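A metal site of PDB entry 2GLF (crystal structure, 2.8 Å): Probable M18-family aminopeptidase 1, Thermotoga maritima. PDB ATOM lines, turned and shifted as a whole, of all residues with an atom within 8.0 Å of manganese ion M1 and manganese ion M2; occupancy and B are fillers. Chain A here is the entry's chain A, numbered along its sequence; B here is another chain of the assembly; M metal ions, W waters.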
ATOM      1  N   ALA A  91       9.006 -10.870  -7.422  1.00  0.00           N
ATOM      2  CA  ALA A  91       9.634  -9.781  -6.685  1.00  0.00           C
ATOM      3  C   ALA A  91      10.249 -10.294  -5.383  1.00  0.00           C
ATOM      4  O   ALA A  91      10.115 -11.469  -5.041  1.00  0.00           O
ATOM      5  CB  ALA A  91       8.618  -8.700  -6.389  1.00  0.00           C
ATOM      6  N   HIS A  92      10.943  -9.417  -4.671  1.00  0.00           N
ATOM      7  CA  HIS A  92      11.552  -9.793  -3.400  1.00  0.00           C
ATOM      8  C   HIS A  92      10.970  -8.936  -2.275  1.00  0.00           C
ATOM      9  O   HIS A  92      10.623  -7.777  -2.483  1.00  0.00           O
ATOM     10  CB  HIS A  92      13.086  -9.678  -3.469  1.00  0.00           C
ATOM     11  CG  HIS A  92      13.605  -8.268  -3.549  1.00  0.00           C
ATOM     12  ND1 HIS A  92      13.928  -7.531  -2.429  1.00  0.00           N
ATOM     13  CD2 HIS A  92      13.952  -7.505  -4.616  1.00  0.00           C
ATOM     14  CE1 HIS A  92      14.449  -6.375  -2.811  1.00  0.00           C
ATOM     15  NE2 HIS A  92      14.470  -6.335  -4.123  1.00  0.00           N
ATOM     16  N   ASP A  94      12.538  -8.753   0.890  1.00  0.00           N
ATOM     17  CA  ASP A  94      13.536  -8.424   1.895  1.00  0.00           C
ATOM     18  C   ASP A  94      14.063  -7.023   1.538  1.00  0.00           C
ATOM     19  O   ASP A  94      14.071  -6.648   0.365  1.00  0.00           O
ATOM     20  CB  ASP A  94      14.689  -9.427   1.885  1.00  0.00           C
ATOM     21  CG  ASP A  94      15.437  -9.447   0.573  1.00  0.00           C
ATOM     22  OD1 ASP A  94      16.680  -9.418   0.600  1.00  0.00           O
ATOM     23  OD2 ASP A  94      14.773  -9.491  -0.496  1.00  0.00           O
ATOM     24  N   SER A  95      14.474  -6.249   2.540  1.00  0.00           N
ATOM     25  CA  SER A  95      14.990  -4.903   2.308  1.00  0.00           C
ATOM     26  C   SER A  95      16.190  -4.597   3.185  1.00  0.00           C
ATOM     27  O   SER A  95      16.322  -5.129   4.278  1.00  0.00           O
ATOM     28  CB  SER A  95      13.911  -3.867   2.596  1.00  0.00           C
ATOM     29  OG  SER A  95      12.898  -3.890   1.620  1.00  0.00           O
ATOM     30  N   PRO A  96      17.101  -3.727   2.701  1.00  0.00           N
ATOM     31  CA  PRO A  96      18.259  -3.418   3.545  1.00  0.00           C
ATOM     32  C   PRO A  96      17.776  -3.060   4.947  1.00  0.00           C
ATOM     33  O   PRO A  96      16.746  -2.403   5.135  1.00  0.00           O
ATOM     34  CB  PRO A  96      18.897  -2.243   2.799  1.00  0.00           C
ATOM     35  CG  PRO A  96      18.690  -2.645   1.359  1.00  0.00           C
ATOM     36  CD  PRO A  96      17.236  -3.112   1.364  1.00  0.00           C
ATOM     37  N   GLY A 120      22.404  -6.180   3.529  1.00  0.00           N
ATOM     38  CA  GLY A 120      22.239  -5.528   2.243  1.00  0.00           C
ATOM     39  C   GLY A 120      23.044  -4.251   2.054  1.00  0.00           C
ATOM     40  O   GLY A 120      23.893  -3.908   2.885  1.00  0.00           O
ATOM     41  N   GLY A 121      22.742  -3.535   0.982  1.00  0.00           N
ATOM     42  CA  GLY A 121      23.450  -2.304   0.673  1.00  0.00           C
ATOM     43  C   GLY A 121      22.958  -1.005   1.276  1.00  0.00           C
ATOM     44  O   GLY A 121      22.608  -0.081   0.549  1.00  0.00           O
ATOM     45  N   GLN A 248      10.388   0.510   0.118  1.00  0.00           N
ATOM     46  CA  GLN A 248       9.636   0.520  -1.124  1.00  0.00           C
ATOM     47  C   GLN A 248      10.406  -0.293  -2.143  1.00  0.00           C
ATOM     48  O   GLN A 248       9.846  -0.745  -3.138  1.00  0.00           O
ATOM     49  CB  GLN A 248       9.426   1.939  -1.629  1.00  0.00           C
ATOM     50  CG  GLN A 248       8.182   2.580  -1.050  1.00  0.00           C
ATOM     51  CD  GLN A 248       7.898   3.939  -1.632  1.00  0.00           C
ATOM     52  OE1 GLN A 248       8.646   4.889  -1.410  1.00  0.00           O
ATOM     53  NE2 GLN A 248       6.818   4.031  -2.400  1.00  0.00           N
ATOM     54  N   ASP A 249      11.703  -0.493  -1.875  1.00  0.00           N
ATOM     55  CA  ASP A 249      12.517  -1.282  -2.783  1.00  0.00           C
ATOM     56  C   ASP A 249      11.923  -2.677  -2.843  1.00  0.00           C
ATOM     57  O   ASP A 249      12.207  -3.546  -2.018  1.00  0.00           O
ATOM     58  CB  ASP A 249      13.966  -1.379  -2.344  1.00  0.00           C
ATOM     59  CG  ASP A 249      14.856  -2.056  -3.395  1.00  0.00           C
ATOM     60  OD1 ASP A 249      14.401  -3.008  -4.059  1.00  0.00           O
ATOM     61  OD2 ASP A 249      16.026  -1.653  -3.549  1.00  0.00           O
ATOM     62  N   ASP A 250      11.055  -2.835  -3.841  1.00  0.00           N
ATOM     63  CA  ASP A 250      10.350  -4.040  -4.199  1.00  0.00           C
ATOM     64  C   ASP A 250       9.097  -4.460  -3.469  1.00  0.00           C
ATOM     65  O   ASP A 250       8.392  -5.354  -3.949  1.00  0.00           O
ATOM     66  CB  ASP A 250      11.303  -5.214  -4.273  1.00  0.00           C
ATOM     67  CG  ASP A 250      11.155  -5.943  -5.570  1.00  0.00           C
ATOM     68  OD1 ASP A 250      11.013  -5.243  -6.603  1.00  0.00           O
ATOM     69  OD2 ASP A 250      11.158  -7.184  -5.574  1.00  0.00           O
ATOM     70  N   ARG A 251       8.787  -3.873  -2.318  1.00  0.00           N
ATOM     71  CA  ARG A 251       7.530  -4.245  -1.695  1.00  0.00           C
ATOM     72  C   ARG A 251       6.499  -3.476  -2.508  1.00  0.00           C
ATOM     73  O   ARG A 251       5.307  -3.776  -2.477  1.00  0.00           O
ATOM     74  CB  ARG A 251       7.478  -3.846  -0.211  1.00  0.00           C
ATOM     75  CG  ARG A 251       8.560  -4.517   0.615  1.00  0.00           C
ATOM     76  CD  ARG A 251       8.148  -4.765   2.056  1.00  0.00           C
ATOM     77  NE  ARG A 251       9.145  -5.602   2.716  1.00  0.00           N
ATOM     78  CZ  ARG A 251      10.179  -5.148   3.416  1.00  0.00           C
ATOM     79  NH1 ARG A 251      10.355  -3.849   3.569  1.00  0.00           N
ATOM     80  NH2 ARG A 251      11.043  -5.996   3.952  1.00  0.00           N
ATOM     81  N   CYS A 253       6.686  -3.439  -5.692  1.00  0.00           N
ATOM     82  CA  CYS A 253       6.445  -4.333  -6.807  1.00  0.00           C
ATOM     83  C   CYS A 253       5.690  -5.550  -6.312  1.00  0.00           C
ATOM     84  O   CYS A 253       4.941  -6.171  -7.063  1.00  0.00           O
ATOM     85  CB  CYS A 253       7.751  -4.754  -7.457  1.00  0.00           C
ATOM     86  SG  CYS A 253       8.320  -3.518  -8.585  1.00  0.00           S
ATOM     87  N   GLU A 278      17.205 -11.470  -1.632  1.00  0.00           N
ATOM     88  CA  GLU A 278      17.690 -10.913  -2.893  1.00  0.00           C
ATOM     89  C   GLU A 278      18.750  -9.846  -2.628  1.00  0.00           C
ATOM     90  O   GLU A 278      19.769  -9.793  -3.325  1.00  0.00           O
ATOM     91  CB  GLU A 278      16.551 -10.289  -3.706  1.00  0.00           C
ATOM     92  CG  GLU A 278      16.635  -8.776  -3.822  1.00  0.00           C
ATOM     93  CD  GLU A 278      17.582  -8.295  -4.887  1.00  0.00           C
ATOM     94  OE1 GLU A 278      17.818  -7.064  -4.958  1.00  0.00           O
ATOM     95  OE2 GLU A 278      18.080  -9.132  -5.672  1.00  0.00           O
ATOM     96  N   GLU A 279      18.497  -9.003  -1.627  1.00  0.00           N
ATOM     97  CA  GLU A 279      19.417  -7.926  -1.271  1.00  0.00           C
ATOM     98  C   GLU A 279      20.820  -8.397  -0.872  1.00  0.00           C
ATOM     99  O   GLU A 279      21.676  -7.569  -0.589  1.00  0.00           O
ATOM    100  CB  GLU A 279      18.830  -7.075  -0.131  1.00  0.00           C
ATOM    101  CG  GLU A 279      17.624  -6.216  -0.483  1.00  0.00           C
ATOM    102  CD  GLU A 279      17.920  -5.122  -1.498  1.00  0.00           C
ATOM    103  OE1 GLU A 279      19.089  -4.916  -1.852  1.00  0.00           O
ATOM    104  OE2 GLU A 279      16.972  -4.464  -1.957  1.00  0.00           O
ATOM    105  N   ILE A 280      21.045  -9.711  -0.813  1.00  0.00           N
ATOM    106  CA  ILE A 280      22.370 -10.222  -0.466  1.00  0.00           C
ATOM    107  C   ILE A 280      22.874 -11.239  -1.494  1.00  0.00           C
ATOM    108  O   ILE A 280      23.860 -11.935  -1.253  1.00  0.00           O
ATOM    109  CB  ILE A 280      22.413 -10.873   0.967  1.00  0.00           C
ATOM    110  CG1 ILE A 280      21.352 -11.961   1.135  1.00  0.00           C
ATOM    111  CG2 ILE A 280      22.239  -9.797   2.021  1.00  0.00           C
ATOM    112  CD1 ILE A 280      21.727 -13.315   0.520  1.00  0.00           C
ATOM    113  N   GLY A 325       9.765  -8.179 -11.377  1.00  0.00           N
ATOM    114  CA  GLY A 325       9.284  -6.946 -10.785  1.00  0.00           C
ATOM    115  C   GLY A 325      10.194  -6.319  -9.749  1.00  0.00           C
ATOM    116  O   GLY A 325      10.168  -6.695  -8.570  1.00  0.00           O
ATOM    117  N   ASP A 326      11.003  -5.349 -10.175  1.00  0.00           N
ATOM    118  CA  ASP A 326      11.919  -4.652  -9.279  1.00  0.00           C
ATOM    119  C   ASP A 326      12.011  -3.185  -9.713  1.00  0.00           C
ATOM    120  O   ASP A 326      11.714  -2.847 -10.860  1.00  0.00           O
ATOM    121  CB  ASP A 326      13.290  -5.308  -9.277  1.00  0.00           C
ATOM    122  CG  ASP A 326      14.057  -5.063  -7.983  1.00  0.00           C
ATOM    123  OD1 ASP A 326      15.088  -5.738  -7.764  1.00  0.00           O
ATOM    124  OD2 ASP A 326      13.637  -4.208  -7.183  1.00  0.00           O
ATOM    125  N   VAL A 327      12.431  -2.324  -8.804  1.00  0.00           N
ATOM    126  CA  VAL A 327      12.527  -0.890  -9.059  1.00  0.00           C
ATOM    127  C   VAL A 327      13.804  -0.439  -9.741  1.00  0.00           C
ATOM    128  O   VAL A 327      14.842  -1.088  -9.634  1.00  0.00           O
ATOM    129  CB  VAL A 327      12.428  -0.095  -7.739  1.00  0.00           C
ATOM    130  CG1 VAL A 327      11.124  -0.419  -7.021  1.00  0.00           C
ATOM    131  CG2 VAL A 327      13.617  -0.442  -6.859  1.00  0.00           C
ATOM    132  N   CYS A 328      13.721   0.680 -10.455  1.00  0.00           N
ATOM    133  CA  CYS A 328      14.895   1.240 -11.116  1.00  0.00           C
ATOM    134  C   CYS A 328      15.109   2.612 -10.491  1.00  0.00           C
ATOM    135  O   CYS A 328      14.361   3.021  -9.599  1.00  0.00           O
ATOM    136  CB  CYS A 328      14.653   1.376 -12.623  1.00  0.00           C
ATOM    137  SG  CYS A 328      13.198   2.353 -13.049  1.00  0.00           S
ATOM    138  N   GLY A 400      23.990  -3.416 -10.854  1.00  0.00           N
ATOM    139  CA  GLY A 400      22.628  -3.666 -10.449  1.00  0.00           C
ATOM    140  C   GLY A 400      22.388  -5.143 -10.224  1.00  0.00           C
ATOM    141  O   GLY A 400      22.615  -5.647  -9.125  1.00  0.00           O
ATOM    142  N   GLY A 401      21.960  -5.839 -11.273  1.00  0.00           N
ATOM    143  CA  GLY A 401      21.705  -7.260 -11.155  1.00  0.00           C
ATOM    144  C   GLY A 401      20.463  -7.550 -10.335  1.00  0.00           C
ATOM    145  O   GLY A 401      20.423  -7.258  -9.135  1.00  0.00           O
ATOM    146  N   THR A 402      19.443  -8.120 -10.972  1.00  0.00           N
ATOM    147  CA  THR A 402      18.205  -8.467 -10.286  1.00  0.00           C
ATOM    148  C   THR A 402      18.042  -9.981 -10.325  1.00  0.00           C
ATOM    149  O   THR A 402      18.910 -10.679 -10.839  1.00  0.00           O
ATOM    150  CB  THR A 402      16.982  -7.828 -10.958  1.00  0.00           C
ATOM    151  OG1 THR A 402      16.917  -8.256 -12.318  1.00  0.00           O
ATOM    152  CG2 THR A 402      17.055  -6.312 -10.905  1.00  0.00           C
ATOM    153  N   ILE A 403      16.928 -10.471  -9.797  1.00  0.00           N
ATOM    154  CA  ILE A 403      16.696 -11.912  -9.778  1.00  0.00           C
ATOM    155  C   ILE A 403      16.256 -12.486 -11.117  1.00  0.00           C
ATOM    156  O   ILE A 403      16.147 -13.702 -11.276  1.00  0.00           O
ATOM    157  CB  ILE A 403      15.666 -12.293  -8.695  1.00  0.00           C
ATOM    158  CG1 ILE A 403      14.261 -11.847  -9.105  1.00  0.00           C
ATOM    159  CG2 ILE A 403      16.044 -11.649  -7.376  1.00  0.00           C
ATOM    160  CD1 ILE A 403      13.170 -12.352  -8.167  1.00  0.00           C
ATOM    161  N   LEU A 421      12.554   4.891  -8.558  1.00  0.00           N
ATOM    162  CA  LEU A 421      12.620   5.465  -7.210  1.00  0.00           C
ATOM    163  C   LEU A 421      13.743   6.473  -7.020  1.00  0.00           C
ATOM    164  O   LEU A 421      14.758   6.444  -7.705  1.00  0.00           O
ATOM    165  CB  LEU A 421      12.800   4.375  -6.146  1.00  0.00           C
ATOM    166  CG  LEU A 421      11.820   3.231  -5.959  1.00  0.00           C
ATOM    167  CD1 LEU A 421      12.250   2.443  -4.752  1.00  0.00           C
ATOM    168  CD2 LEU A 421      10.410   3.757  -5.765  1.00  0.00           C
ATOM    169  N   MET A 424      16.909   5.247  -3.468  1.00  0.00           N
ATOM    170  CA  MET A 424      16.779   3.804  -3.255  1.00  0.00           C
ATOM    171  C   MET A 424      17.717   3.380  -2.116  1.00  0.00           C
ATOM    172  O   MET A 424      18.829   3.879  -2.002  1.00  0.00           O
ATOM    173  CB  MET A 424      17.108   3.057  -4.539  1.00  0.00           C
ATOM    174  CG  MET A 424      16.595   1.616  -4.582  1.00  0.00           C
ATOM    175  SD  MET A 424      16.993   0.717  -6.271  1.00  0.00           S
ATOM    176  CE  MET A 424      18.041  -0.777  -5.614  1.00  0.00           C
ATOM    177  N   HIS A 425      17.243   2.465  -1.276  1.00  0.00           N
ATOM    178  CA  HIS A 425      17.981   1.942  -0.118  1.00  0.00           C
ATOM    179  C   HIS A 425      18.072   2.856   1.089  1.00  0.00           C
ATOM    180  O   HIS A 425      18.564   2.441   2.143  1.00  0.00           O
ATOM    181  CB  HIS A 425      19.387   1.494  -0.519  1.00  0.00           C
ATOM    182  CG  HIS A 425      19.416   0.184  -1.228  1.00  0.00           C
ATOM    183  ND1 HIS A 425      20.539  -0.601  -1.304  1.00  0.00           N
ATOM    184  CD2 HIS A 425      18.448  -0.491  -1.883  1.00  0.00           C
ATOM    185  CE1 HIS A 425      20.261  -1.705  -1.959  1.00  0.00           C
ATOM    186  NE2 HIS A 425      18.992  -1.664  -2.329  1.00  0.00           N
ATOM    187  N   GLU A 429      12.563   5.942   1.009  1.00  0.00           N
ATOM    188  CA  GLU A 429      12.561   5.993  -0.446  1.00  0.00           C
ATOM    189  C   GLU A 429      11.349   6.750  -0.967  1.00  0.00           C
ATOM    190  O   GLU A 429      10.326   6.848  -0.296  1.00  0.00           O
ATOM    191  CB  GLU A 429      12.583   4.578  -1.023  1.00  0.00           C
ATOM    192  CG  GLU A 429      13.738   3.739  -0.497  1.00  0.00           C
ATOM    193  CD  GLU A 429      13.696   2.303  -0.980  1.00  0.00           C
ATOM    194  OE1 GLU A 429      12.598   1.703  -0.993  1.00  0.00           O
ATOM    195  OE2 GLU A 429      14.766   1.747  -1.330  1.00  0.00           O
ATOM    196  N   PRO B 166      22.936   4.163  -3.487  1.00  0.00           N
ATOM    197  CA  PRO B 166      24.325   3.722  -3.397  1.00  0.00           C
ATOM    198  C   PRO B 166      24.861   2.975  -4.618  1.00  0.00           C
ATOM    199  O   PRO B 166      26.068   2.829  -4.769  1.00  0.00           O
ATOM    200  CB  PRO B 166      24.316   2.855  -2.132  1.00  0.00           C
ATOM    201  CG  PRO B 166      22.923   2.319  -2.106  1.00  0.00           C
ATOM    202  CD  PRO B 166      22.100   3.516  -2.457  1.00  0.00           C
ATOM    203  N   HIS B 167      23.970   2.533  -5.499  1.00  0.00           N
ATOM    204  CA  HIS B 167      24.354   1.800  -6.704  1.00  0.00           C
ATOM    205  C   HIS B 167      25.037   2.651  -7.758  1.00  0.00           C
ATOM    206  O   HIS B 167      25.815   2.147  -8.567  1.00  0.00           O
ATOM    207  CB  HIS B 167      23.123   1.171  -7.356  1.00  0.00           C
ATOM    208  CG  HIS B 167      22.217   0.481  -6.388  1.00  0.00           C
ATOM    209  ND1 HIS B 167      22.331  -0.862  -6.085  1.00  0.00           N
ATOM    210  CD2 HIS B 167      21.220   0.950  -5.614  1.00  0.00           C
ATOM    211  CE1 HIS B 167      21.433  -1.186  -5.174  1.00  0.00           C
ATOM    212  NE2 HIS B 167      20.743  -0.107  -4.872  1.00  0.00           N
HETATM  213 MN    MN M   1      17.724  -3.364  -3.497  1.00  0.00          MN
HETATM  214 MN    MN M   2      15.337  -4.529  -5.527  1.00  0.00          MN
HETATM  215  O   HOH W   1      15.731  -2.535  -6.734  1.00  0.00           O
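Water W1 lies within hydrogen-bond range of O of Val 327 (3.4 Å) and SD of Met 424 (3.5 Å).
Merely in contact with manganese ion M2: Glu 278.
Within 4 Å of manganese ion M2: His 92, Asp 249, Glu 278, Glu 279 and Asp 326.
Residues that only touch manganese ion M1: Met 424 (3.4 Å) and Glu 278 (3.98 Å).
The nearest printed residue that does not touch manganese ion M1 is His 92 (4.5 Å).
A ring nitrogen (NE2) of His 167 of chain B lies close to a ring nitrogen (NE2) of His 425.
The side-chain carboxylate (OD1) of Asp 94 is in hydrogen-bond range of the backbone NH (N) of Glu 278 (3.1 Å).
A ring nitrogen (ND1) of His 92 sits at hydrogen-bond distance from the side-chain carboxylate of Asp 94 (2.9 Å).
N of His 92 lies within hydrogen-bond range of OD2 of Asp 250 (2.4 Å).
The side-chain carboxylate of Glu 429 lies within hydrogen-bond range of the backbone NH of Asp 249, 2.5 Å away.
The backbone NH (N) of Asp 326 sits at hydrogen-bond distance from the side-chain sulfur (SG) of Cys 253 (3.6 Å).
OE2 of Glu 429 is in hydrogen-bond range of N of His 425, at 2.6 Å.
ND1 of His 425 is in hydrogen-bond range of O of Gly 121 (2.8 Å).
Manganese ion M1 is bound by the side-chain carboxylate (OE2) of Glu 279 (2.0 Å), the side-chain carboxylate (OD2) of Asp 249 (2.4 Å), a ring nitrogen (NE2) of His 425 (2.4 Å) and the side-chain carboxylate (OE1) of Glu 279 (2.6 Å).
Manganese ion M1 has four donor atoms within binding distance.
Manganese ion M2 is bound by OD1 of Asp 249 (2.3 Å), water W1 (2.4 Å), OD2 of Asp 326 (2.4 Å), NE2 of His 92 (2.4 Å) and OD1 of Asp 326 (2.6 Å).
Manganese ion M2 has five donor atoms within binding distance.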
